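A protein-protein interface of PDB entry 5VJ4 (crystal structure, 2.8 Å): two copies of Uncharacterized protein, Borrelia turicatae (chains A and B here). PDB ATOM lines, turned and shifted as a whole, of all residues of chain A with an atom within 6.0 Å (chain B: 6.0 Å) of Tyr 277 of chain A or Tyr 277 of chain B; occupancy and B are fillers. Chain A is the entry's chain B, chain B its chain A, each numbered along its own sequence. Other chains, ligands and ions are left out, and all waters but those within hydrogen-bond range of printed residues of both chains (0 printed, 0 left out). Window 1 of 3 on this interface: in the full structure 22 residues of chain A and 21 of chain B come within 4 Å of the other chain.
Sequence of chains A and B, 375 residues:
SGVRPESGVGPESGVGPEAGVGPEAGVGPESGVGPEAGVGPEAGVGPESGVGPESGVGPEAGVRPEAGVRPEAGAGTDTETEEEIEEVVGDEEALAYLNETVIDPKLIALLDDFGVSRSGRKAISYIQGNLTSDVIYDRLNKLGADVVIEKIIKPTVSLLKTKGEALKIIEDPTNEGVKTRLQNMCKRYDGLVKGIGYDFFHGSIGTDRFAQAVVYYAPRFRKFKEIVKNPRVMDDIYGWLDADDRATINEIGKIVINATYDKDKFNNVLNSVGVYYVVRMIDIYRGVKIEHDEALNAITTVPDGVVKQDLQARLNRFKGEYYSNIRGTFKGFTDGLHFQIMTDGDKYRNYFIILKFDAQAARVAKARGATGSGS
Tyr 276 of chain A touches Phe 333 of chain B, and with the chains exchanged Phe 333 of chain A touches Tyr 276 of chain B. Tyr 277 of chain A touches its own counterpart, Tyr 277 of chain B. Tyr 277 of chain A touches Gln 340 of chain B, and with the chains exchanged Gln 340 of chain A touches Tyr 277 of chain B. Arg 280 of chain A touches Phe 339 of chain B, and with the chains exchanged Phe 339 of chain A touches Arg 280 of chain B. Of the 16 pairs that touch across the chains among the printed residues, 16 have their exchanged pair printed and touching as well.
Of the 15 printed residues of chain A, 8 touch a printed residue of chain B. Of the 15 printed residues of chain B, 8 touch a printed residue of chain A. Hydrophobic or aromatic side chains of chain B that line the printed part of chain A: Val 273, Tyr 276, Tyr 277, Phe 333 and Phe 339.
Among the printed residues, merely in contact across the chains: Tyr 276 of chain A with Phe 339 of chain B, Arg 280 of chain A with Phe 339 of chain B, Phe 339 of chain A with Arg 280 of chain B, Phe 333 of chain A with Tyr 276 of chain B, Phe 339 of chain A with Tyr 276 of chain B, Tyr 276 of chain A with Phe 333 of chain B, Tyr 277 of chain A with Val 273 of chain B, Tyr 277 of chain A with Tyr 277 of chain B, Val 273 of chain A with Tyr 277 of chain B, Ser 272 of chain A with Tyr 276 of chain B, Tyr 276 of chain A with Ser 272 of chain B and Tyr 277 of chain A with Gln 340 of chain B.
Val 275 of chain A touches none of the printed residues of chain B. Of the printed residues of chain B, Tyr 276 of chain A touches Ser 272, Phe 333 and Phe 339. Of chain B, only Val 273, Tyr 277, Phe 339 and Gln 340 come within 4 Å of Tyr 277 of chain A. Tyr 277 of chain B touches just these residues of chain A: Val 273 (3.4 Å), Tyr 277 (3.4 Å), Phe 339 (2.7 Å) and Gln 340 (2.7 Å). Of the printed residues of chain A, Gln 340 of chain B touches Tyr 277 and Gln 340. The nearest residue of chain A that does not touch Tyr 277 of chain B is Phe 333 of chain A (4.6 Å). The nearest printed residue of chain B that does not touch Phe 333 of chain A is Tyr 277 of chain B (4.6 Å).
The backbone carbonyl oxygen (O) of Phe 339 of chain A is in hydrogen-bond range of the side-chain hydroxyl (OH) of Tyr 277 of chain B. The side-chain hydroxyl (OH) of Tyr 277 of chain B is in hydrogen-bond range of the side-chain amide oxygen (OE1) of Gln 340 of chain A (2.7 Å). The backbone carbonyl oxygen of Phe 339 of chain B lies within hydrogen-bond range of the side-chain hydroxyl of Tyr 277 of chain A (2.6 Å). The side-chain amide oxygen (OE1) of Gln 340 of chain B sits close to the side-chain amide oxygen (OE1) of Gln 340 of chain A, 2.8 Å away.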
ATOM      1  N   SER A 272       5.773 -35.122   5.082  1.00  0.00           N
ATOM      2  CA  SER A 272       5.617 -34.011   4.137  1.00  0.00           C
ATOM      3  C   SER A 272       4.924 -32.829   4.768  1.00  0.00           C
ATOM      4  O   SER A 272       5.371 -31.687   4.601  1.00  0.00           O
ATOM      5  CB  SER A 272       4.907 -34.442   2.849  1.00  0.00           C
ATOM      6  OG  SER A 272       5.608 -35.534   2.264  1.00  0.00           O
ATOM      7  N   VAL A 273       3.852 -33.094   5.511  1.00  0.00           N
ATOM      8  CA  VAL A 273       3.069 -31.993   6.037  1.00  0.00           C
ATOM      9  C   VAL A 273       3.756 -31.331   7.229  1.00  0.00           C
ATOM     10  O   VAL A 273       3.664 -30.107   7.405  1.00  0.00           O
ATOM     11  CB  VAL A 273       1.638 -32.414   6.349  1.00  0.00           C
ATOM     12  CG1 VAL A 273       1.019 -32.938   5.072  1.00  0.00           C
ATOM     13  CG2 VAL A 273       1.579 -33.483   7.422  1.00  0.00           C
ATOM     14  N   GLY A 274       4.481 -32.132   8.012  1.00  0.00           N
ATOM     15  CA  GLY A 274       5.187 -31.628   9.193  1.00  0.00           C
ATOM     16  C   GLY A 274       4.402 -31.733  10.489  1.00  0.00           C
ATOM     17  O   GLY A 274       3.186 -31.981  10.493  1.00  0.00           O
ATOM     18  N   VAL A 275       5.097 -31.528  11.599  1.00  0.00           N
ATOM     19  CA  VAL A 275       4.475 -31.677  12.913  1.00  0.00           C
ATOM     20  C   VAL A 275       3.244 -30.784  13.053  1.00  0.00           C
ATOM     21  O   VAL A 275       2.208 -31.245  13.534  1.00  0.00           O
ATOM     22  CB  VAL A 275       5.474 -31.361  14.025  1.00  0.00           C
ATOM     23  CG1 VAL A 275       4.782 -31.336  15.377  1.00  0.00           C
ATOM     24  CG2 VAL A 275       6.633 -32.355  14.000  1.00  0.00           C
ATOM     25  N   TYR A 276       3.359 -29.531  12.595  1.00  0.00           N
ATOM     26  CA  TYR A 276       2.276 -28.571  12.686  1.00  0.00           C
ATOM     27  C   TYR A 276       0.946 -29.222  12.232  1.00  0.00           C
ATOM     28  O   TYR A 276      -0.007 -29.342  13.020  1.00  0.00           O
ATOM     29  CB  TYR A 276       2.647 -27.318  11.882  1.00  0.00           C
ATOM     30  CG  TYR A 276       1.631 -26.190  11.934  1.00  0.00           C
ATOM     31  CD1 TYR A 276       1.506 -25.402  13.056  1.00  0.00           C
ATOM     32  CD2 TYR A 276       0.814 -25.901  10.852  1.00  0.00           C
ATOM     33  CE1 TYR A 276       0.605 -24.353  13.108  1.00  0.00           C
ATOM     34  CE2 TYR A 276      -0.094 -24.856  10.908  1.00  0.00           C
ATOM     35  CZ  TYR A 276      -0.187 -24.080  12.035  1.00  0.00           C
ATOM     36  OH  TYR A 276      -1.096 -23.047  12.101  1.00  0.00           O
ATOM     37  N   TYR A 277       0.926 -29.710  10.989  1.00  0.00           N
ATOM     38  CA  TYR A 277      -0.282 -30.282  10.441  1.00  0.00           C
ATOM     39  C   TYR A 277      -0.640 -31.628  11.023  1.00  0.00           C
ATOM     40  O   TYR A 277      -1.820 -31.932  11.214  1.00  0.00           O
ATOM     41  CB  TYR A 277      -0.217 -30.322   8.947  1.00  0.00           C
ATOM     42  CG  TYR A 277      -0.286 -28.952   8.399  1.00  0.00           C
ATOM     43  CD1 TYR A 277      -1.454 -28.236   8.486  1.00  0.00           C
ATOM     44  CD2 TYR A 277       0.841 -28.346   7.809  1.00  0.00           C
ATOM     45  CE1 TYR A 277      -1.526 -26.933   8.005  1.00  0.00           C
ATOM     46  CE2 TYR A 277       0.780 -27.056   7.294  1.00  0.00           C
ATOM     47  CZ  TYR A 277      -0.408 -26.354   7.407  1.00  0.00           C
ATOM     48  OH  TYR A 277      -0.498 -25.072   6.944  1.00  0.00           O
ATOM     49  N   VAL A 278       0.379 -32.413  11.334  1.00  0.00           N
ATOM     50  CA  VAL A 278       0.159 -33.702  11.973  1.00  0.00           C
ATOM     51  C   VAL A 278      -0.633 -33.539  13.267  1.00  0.00           C
ATOM     52  O   VAL A 278      -1.692 -34.161  13.424  1.00  0.00           O
ATOM     53  CB  VAL A 278       1.473 -34.470  12.233  1.00  0.00           C
ATOM     54  CG1 VAL A 278       1.203 -35.693  13.095  1.00  0.00           C
ATOM     55  CG2 VAL A 278       2.114 -34.896  10.920  1.00  0.00           C
ATOM     56  N   VAL A 279      -0.141 -32.694  14.180  1.00  0.00           N
ATOM     57  CA  VAL A 279      -0.781 -32.593  15.507  1.00  0.00           C
ATOM     58  C   VAL A 279      -2.175 -32.011  15.373  1.00  0.00           C
ATOM     59  O   VAL A 279      -3.099 -32.401  16.089  1.00  0.00           O
ATOM     60  CB  VAL A 279       0.042 -31.825  16.575  1.00  0.00           C
ATOM     61  CG1 VAL A 279       1.414 -32.476  16.815  1.00  0.00           C
ATOM     62  CG2 VAL A 279       0.165 -30.348  16.251  1.00  0.00           C
ATOM     63  N   ARG A 280      -2.349 -31.114  14.416  1.00  0.00           N
ATOM     64  CA  ARG A 280      -3.655 -30.564  14.223  1.00  0.00           C
ATOM     65  C   ARG A 280      -4.616 -31.682  13.846  1.00  0.00           C
ATOM     66  O   ARG A 280      -5.746 -31.738  14.334  1.00  0.00           O
ATOM     67  CB  ARG A 280      -3.625 -29.427  13.206  1.00  0.00           C
ATOM     68  CG  ARG A 280      -4.936 -28.673  13.187  1.00  0.00           C
ATOM     69  CD  ARG A 280      -4.777 -27.383  12.429  1.00  0.00           C
ATOM     70  NE  ARG A 280      -5.989 -27.092  11.671  1.00  0.00           N
ATOM     71  CZ  ARG A 280      -7.159 -26.733  12.202  1.00  0.00           C
ATOM     72  NH1 ARG A 280      -7.308 -26.607  13.517  1.00  0.00           N
ATOM     73  NH2 ARG A 280      -8.190 -26.485  11.400  1.00  0.00           N
ATOM     74  N   MET A 281      -4.148 -32.595  13.003  1.00  0.00           N
ATOM     75  CA  MET A 281      -4.982 -33.711  12.594  1.00  0.00           C
ATOM     76  C   MET A 281      -5.336 -34.546  13.789  1.00  0.00           C
ATOM     77  O   MET A 281      -6.518 -34.822  14.022  1.00  0.00           O
ATOM     78  CB  MET A 281      -4.275 -34.549  11.561  1.00  0.00           C
ATOM     79  CG  MET A 281      -5.062 -35.821  11.242  1.00  0.00           C
ATOM     80  SD  MET A 281      -3.836 -36.903  10.146  1.00  0.00           S
ATOM     81  CE  MET A 281      -2.541 -37.709  11.380  1.00  0.00           C
ATOM     82  N   ILE A 282      -4.312 -34.942  14.543  1.00  0.00           N
ATOM     83  CA  ILE A 282      -4.480 -35.684  15.792  1.00  0.00           C
ATOM     84  C   ILE A 282      -5.626 -35.124  16.668  1.00  0.00           C
ATOM     85  O   ILE A 282      -6.567 -35.825  17.013  1.00  0.00           O
ATOM     86  CB  ILE A 282      -3.169 -35.722  16.604  1.00  0.00           C
ATOM     87  CG1 ILE A 282      -2.063 -36.461  15.836  1.00  0.00           C
ATOM     88  CG2 ILE A 282      -3.425 -36.360  17.962  1.00  0.00           C
ATOM     89  CD1 ILE A 282      -0.968 -37.053  16.711  1.00  0.00           C
ATOM     90  N   PHE A 333      -3.337 -37.714  -1.234  1.00  0.00           N
ATOM     91  CA  PHE A 333      -2.080 -37.055  -0.934  1.00  0.00           C
ATOM     92  C   PHE A 333      -0.941 -37.779  -1.636  1.00  0.00           C
ATOM     93  O   PHE A 333      -0.145 -37.144  -2.326  1.00  0.00           O
ATOM     94  CB  PHE A 333      -1.817 -36.972   0.575  1.00  0.00           C
ATOM     95  CG  PHE A 333      -0.750 -35.979   0.944  1.00  0.00           C
ATOM     96  CD1 PHE A 333       0.601 -36.300   0.777  1.00  0.00           C
ATOM     97  CD2 PHE A 333      -1.096 -34.698   1.426  1.00  0.00           C
ATOM     98  CE1 PHE A 333       1.595 -35.381   1.097  1.00  0.00           C
ATOM     99  CE2 PHE A 333      -0.111 -33.789   1.741  1.00  0.00           C
ATOM    100  CZ  PHE A 333       1.238 -34.128   1.577  1.00  0.00           C
ATOM    101  N   PHE A 339      -2.364 -31.528  -1.480  1.00  0.00           N
ATOM    102  CA  PHE A 339      -1.174 -31.392  -0.639  1.00  0.00           C
ATOM    103  C   PHE A 339      -1.528 -31.085   0.795  1.00  0.00           C
ATOM    104  O   PHE A 339      -0.728 -30.587   1.571  1.00  0.00           O
ATOM    105  CB  PHE A 339      -0.195 -30.411  -1.265  1.00  0.00           C
ATOM    106  CG  PHE A 339       0.076 -30.720  -2.698  1.00  0.00           C
ATOM    107  CD1 PHE A 339       1.079 -31.609  -3.056  1.00  0.00           C
ATOM    108  CD2 PHE A 339      -0.755 -30.199  -3.690  1.00  0.00           C
ATOM    109  CE1 PHE A 339       1.275 -31.931  -4.387  1.00  0.00           C
ATOM    110  CE2 PHE A 339      -0.552 -30.515  -5.022  1.00  0.00           C
ATOM    111  CZ  PHE A 339       0.469 -31.368  -5.370  1.00  0.00           C
ATOM    112  N   GLN A 340      -2.730 -31.483   1.159  1.00  0.00           N
ATOM    113  CA  GLN A 340      -3.220 -31.215   2.468  1.00  0.00           C
ATOM    114  C   GLN A 340      -4.088 -32.335   3.029  1.00  0.00           C
ATOM    115  O   GLN A 340      -5.009 -32.776   2.358  1.00  0.00           O
ATOM    116  CB  GLN A 340      -4.021 -29.906   2.443  1.00  0.00           C
ATOM    117  CG  GLN A 340      -4.327 -29.496   3.859  1.00  0.00           C
ATOM    118  CD  GLN A 340      -3.054 -29.448   4.727  1.00  0.00           C
ATOM    119  OE1 GLN A 340      -2.107 -28.720   4.403  1.00  0.00           O
ATOM    120  NE2 GLN A 340      -3.023 -30.230   5.823  1.00  0.00           N
ATOM    121  N   ILE A 341      -3.831 -32.756   4.265  1.00  0.00           N
ATOM    122  CA  ILE A 341      -4.726 -33.690   4.957  1.00  0.00           C
ATOM    123  C   ILE A 341      -5.958 -32.962   5.453  1.00  0.00           C
ATOM    124  O   ILE A 341      -5.862 -32.079   6.308  1.00  0.00           O
ATOM    125  CB  ILE A 341      -4.030 -34.369   6.130  1.00  0.00           C
ATOM    126  CG1 ILE A 341      -2.979 -35.327   5.598  1.00  0.00           C
ATOM    127  CG2 ILE A 341      -5.038 -35.129   6.987  1.00  0.00           C
ATOM    128  CD1 ILE A 341      -1.797 -35.400   6.526  1.00  0.00           C
ATOM    129  N   SER B 272       5.540 -21.230  10.236  1.00  0.00           N
ATOM    130  CA  SER B 272       4.640 -22.206  10.844  1.00  0.00           C
ATOM    131  C   SER B 272       4.321 -23.282   9.811  1.00  0.00           C
ATOM    132  O   SER B 272       4.324 -24.502  10.078  1.00  0.00           O
ATOM    133  CB  SER B 272       3.367 -21.534  11.322  1.00  0.00           C
ATOM    134  OG  SER B 272       3.656 -20.298  11.935  1.00  0.00           O
ATOM    135  N   VAL B 273       4.094 -22.792   8.610  1.00  0.00           N
ATOM    136  CA  VAL B 273       3.650 -23.601   7.509  1.00  0.00           C
ATOM    137  C   VAL B 273       4.794 -24.487   6.986  1.00  0.00           C
ATOM    138  O   VAL B 273       4.567 -25.622   6.588  1.00  0.00           O
ATOM    139  CB  VAL B 273       3.104 -22.634   6.445  1.00  0.00           C
ATOM    140  CG1 VAL B 273       3.472 -23.039   5.045  1.00  0.00           C
ATOM    141  CG2 VAL B 273       1.619 -22.471   6.637  1.00  0.00           C
ATOM    142  N   GLY B 274       6.021 -23.976   7.004  1.00  0.00           N
ATOM    143  CA  GLY B 274       7.165 -24.752   6.550  1.00  0.00           C
ATOM    144  C   GLY B 274       7.468 -24.629   5.067  1.00  0.00           C
ATOM    145  O   GLY B 274       6.661 -24.160   4.251  1.00  0.00           O
ATOM    146  N   VAL B 275       8.663 -25.065   4.722  1.00  0.00           N
ATOM    147  CA  VAL B 275       9.135 -24.920   3.363  1.00  0.00           C
ATOM    148  C   VAL B 275       8.250 -25.583   2.313  1.00  0.00           C
ATOM    149  O   VAL B 275       8.092 -25.051   1.224  1.00  0.00           O
ATOM    150  CB  VAL B 275      10.513 -25.521   3.244  1.00  0.00           C
ATOM    151  CG1 VAL B 275      10.985 -25.458   1.812  1.00  0.00           C
ATOM    152  CG2 VAL B 275      11.464 -24.787   4.174  1.00  0.00           C
ATOM    153  N   TYR B 276       7.717 -26.755   2.631  1.00  0.00           N
ATOM    154  CA  TYR B 276       6.861 -27.468   1.716  1.00  0.00           C
ATOM    155  C   TYR B 276       5.715 -26.580   1.254  1.00  0.00           C
ATOM    156  O   TYR B 276       5.524 -26.417   0.048  1.00  0.00           O
ATOM    157  CB  TYR B 276       6.333 -28.681   2.418  1.00  0.00           C
ATOM    158  CG  TYR B 276       5.407 -29.559   1.642  1.00  0.00           C
ATOM    159  CD1 TYR B 276       5.904 -30.488   0.759  1.00  0.00           C
ATOM    160  CD2 TYR B 276       4.032 -29.521   1.849  1.00  0.00           C
ATOM    161  CE1 TYR B 276       5.065 -31.354   0.084  1.00  0.00           C
ATOM    162  CE2 TYR B 276       3.180 -30.377   1.171  1.00  0.00           C
ATOM    163  CZ  TYR B 276       3.710 -31.298   0.299  1.00  0.00           C
ATOM    164  OH  TYR B 276       2.884 -32.139  -0.389  1.00  0.00           O
ATOM    165  N   TYR B 277       4.966 -25.990   2.185  1.00  0.00           N
ATOM    166  CA  TYR B 277       3.879 -25.088   1.741  1.00  0.00           C
ATOM    167  C   TYR B 277       4.353 -23.760   1.194  1.00  0.00           C
ATOM    168  O   TYR B 277       3.684 -23.190   0.351  1.00  0.00           O
ATOM    169  CB  TYR B 277       2.819 -24.853   2.797  1.00  0.00           C
ATOM    170  CG  TYR B 277       2.143 -26.122   3.121  1.00  0.00           C
ATOM    171  CD1 TYR B 277       2.672 -26.994   4.073  1.00  0.00           C
ATOM    172  CD2 TYR B 277       1.013 -26.503   2.426  1.00  0.00           C
ATOM    173  CE1 TYR B 277       2.076 -28.211   4.332  1.00  0.00           C
ATOM    174  CE2 TYR B 277       0.417 -27.713   2.668  1.00  0.00           C
ATOM    175  CZ  TYR B 277       0.955 -28.568   3.613  1.00  0.00           C
ATOM    176  OH  TYR B 277       0.360 -29.782   3.866  1.00  0.00           O
ATOM    177  N   VAL B 278       5.504 -23.285   1.660  1.00  0.00           N
ATOM    178  CA  VAL B 278       5.962 -22.018   1.211  1.00  0.00           C
ATOM    179  C   VAL B 278       6.314 -22.114  -0.260  1.00  0.00           C
ATOM    180  O   VAL B 278       5.883 -21.282  -1.041  1.00  0.00           O
ATOM    181  CB  VAL B 278       7.151 -21.486   2.011  1.00  0.00           C
ATOM    182  CG1 VAL B 278       7.792 -20.306   1.279  1.00  0.00           C
ATOM    183  CG2 VAL B 278       6.684 -21.020   3.365  1.00  0.00           C
ATOM    184  N   VAL B 279       7.088 -23.118  -0.649  1.00  0.00           N
ATOM    185  CA  VAL B 279       7.505 -23.181  -2.056  1.00  0.00           C
ATOM    186  C   VAL B 279       6.327 -23.403  -2.995  1.00  0.00           C
ATOM    187  O   VAL B 279       6.278 -22.835  -4.065  1.00  0.00           O
ATOM    188  CB  VAL B 279       8.628 -24.181  -2.339  1.00  0.00           C
ATOM    189  CG1 VAL B 279       9.846 -23.811  -1.526  1.00  0.00           C
ATOM    190  CG2 VAL B 279       8.224 -25.602  -2.045  1.00  0.00           C
ATOM    191  N   ARG B 280       5.346 -24.181  -2.575  1.00  0.00           N
ATOM    192  CA  ARG B 280       4.211 -24.364  -3.434  1.00  0.00           C
ATOM    193  C   ARG B 280       3.427 -23.064  -3.664  1.00  0.00           C
ATOM    194  O   ARG B 280       3.009 -22.778  -4.771  1.00  0.00           O
ATOM    195  CB  ARG B 280       3.329 -25.450  -2.905  1.00  0.00           C
ATOM    196  CG  ARG B 280       2.290 -25.820  -3.907  1.00  0.00           C
ATOM    197  CD  ARG B 280       1.542 -27.048  -3.473  1.00  0.00           C
ATOM    198  NE  ARG B 280       0.592 -27.401  -4.528  1.00  0.00           N
ATOM    199  CZ  ARG B 280      -0.670 -26.990  -4.555  1.00  0.00           C
ATOM    200  NH1 ARG B 280      -1.446 -27.366  -5.551  1.00  0.00           N
ATOM    201  NH2 ARG B 280      -1.158 -26.211  -3.583  1.00  0.00           N
ATOM    202  N   MET B 281       3.269 -22.258  -2.627  1.00  0.00           N
ATOM    203  CA  MET B 281       2.595 -20.978  -2.791  1.00  0.00           C
ATOM    204  C   MET B 281       3.376 -20.118  -3.735  1.00  0.00           C
ATOM    205  O   MET B 281       2.799 -19.309  -4.419  1.00  0.00           O
ATOM    206  CB  MET B 281       2.514 -20.307  -1.454  1.00  0.00           C
ATOM    207  CG  MET B 281       1.981 -18.902  -1.627  1.00  0.00           C
ATOM    208  SD  MET B 281       2.354 -17.858   0.021  1.00  0.00           S
ATOM    209  CE  MET B 281       4.216 -17.299  -0.166  1.00  0.00           C
ATOM    210  N   ILE B 282       4.685 -20.312  -3.797  1.00  0.00           N
ATOM    211  CA  ILE B 282       5.547 -19.521  -4.684  1.00  0.00           C
ATOM    212  C   ILE B 282       5.334 -19.890  -6.157  1.00  0.00           C
ATOM    213  O   ILE B 282       5.202 -18.989  -7.006  1.00  0.00           O
ATOM    214  CB  ILE B 282       7.056 -19.665  -4.318  1.00  0.00           C
ATOM    215  CG1 ILE B 282       7.318 -19.146  -2.905  1.00  0.00           C
ATOM    216  CG2 ILE B 282       7.954 -18.934  -5.310  1.00  0.00           C
ATOM    217  CD1 ILE B 282       8.775 -19.136  -2.510  1.00  0.00           C
ATOM    218  N   PHE B 333      -4.600 -16.108   8.984  1.00  0.00           N
ATOM    219  CA  PHE B 333      -3.723 -17.095   9.562  1.00  0.00           C
ATOM    220  C   PHE B 333      -3.228 -16.594  10.913  1.00  0.00           C
ATOM    221  O   PHE B 333      -3.433 -17.258  11.916  1.00  0.00           O
ATOM    222  CB  PHE B 333      -2.573 -17.382   8.637  1.00  0.00           C
ATOM    223  CG  PHE B 333      -1.780 -18.583   9.019  1.00  0.00           C
ATOM    224  CD1 PHE B 333      -0.958 -18.578  10.144  1.00  0.00           C
ATOM    225  CD2 PHE B 333      -1.826 -19.728   8.231  1.00  0.00           C
ATOM    226  CE1 PHE B 333      -0.208 -19.692  10.485  1.00  0.00           C
ATOM    227  CE2 PHE B 333      -1.088 -20.856   8.567  1.00  0.00           C
ATOM    228  CZ  PHE B 333      -0.277 -20.843   9.699  1.00  0.00           C
ATOM    229  N   PHE B 339      -5.560 -22.318   9.167  1.00  0.00           N
ATOM    230  CA  PHE B 339      -4.208 -22.852   9.320  1.00  0.00           C
ATOM    231  C   PHE B 339      -3.543 -23.258   8.024  1.00  0.00           C
ATOM    232  O   PHE B 339      -2.600 -24.064   8.026  1.00  0.00           O
ATOM    233  CB  PHE B 339      -4.207 -23.980  10.356  1.00  0.00           C
ATOM    234  CG  PHE B 339      -4.815 -23.573  11.671  1.00  0.00           C
ATOM    235  CD1 PHE B 339      -6.195 -23.688  11.885  1.00  0.00           C
ATOM    236  CD2 PHE B 339      -4.030 -23.014  12.669  1.00  0.00           C
ATOM    237  CE1 PHE B 339      -6.766 -23.292  13.074  1.00  0.00           C
ATOM    238  CE2 PHE B 339      -4.603 -22.609  13.865  1.00  0.00           C
ATOM    239  CZ  PHE B 339      -5.971 -22.752  14.068  1.00  0.00           C
ATOM    240  N   GLN B 340      -4.005 -22.664   6.921  1.00  0.00           N
ATOM    241  CA  GLN B 340      -3.440 -22.942   5.584  1.00  0.00           C
ATOM    242  C   GLN B 340      -3.301 -21.631   4.813  1.00  0.00           C
ATOM    243  O   GLN B 340      -4.250 -20.819   4.806  1.00  0.00           O
ATOM    244  CB  GLN B 340      -4.367 -23.842   4.770  1.00  0.00           C
ATOM    245  CG  GLN B 340      -5.205 -24.882   5.495  1.00  0.00           C
ATOM    246  CD  GLN B 340      -4.649 -26.267   5.322  1.00  0.00           C
ATOM    247  OE1 GLN B 340      -3.806 -26.503   4.449  1.00  0.00           O
ATOM    248  NE2 GLN B 340      -5.106 -27.196   6.161  1.00  0.00           N
ATOM    249  N   ILE B 341      -2.160 -21.413   4.154  1.00  0.00           N
ATOM    250  CA  ILE B 341      -2.089 -20.285   3.236  1.00  0.00           C
ATOM    251  C   ILE B 341      -2.745 -20.726   1.952  1.00  0.00           C
ATOM    252  O   ILE B 341      -2.251 -21.647   1.304  1.00  0.00           O
ATOM    253  CB  ILE B 341      -0.671 -19.926   2.837  1.00  0.00           C
ATOM    254  CG1 ILE B 341       0.171 -19.607   4.036  1.00  0.00           C
ATOM    255  CG2 ILE B 341      -0.688 -18.741   1.878  1.00  0.00           C
ATOM    256  CD1 ILE B 341       1.632 -19.603   3.635  1.00  0.00           C
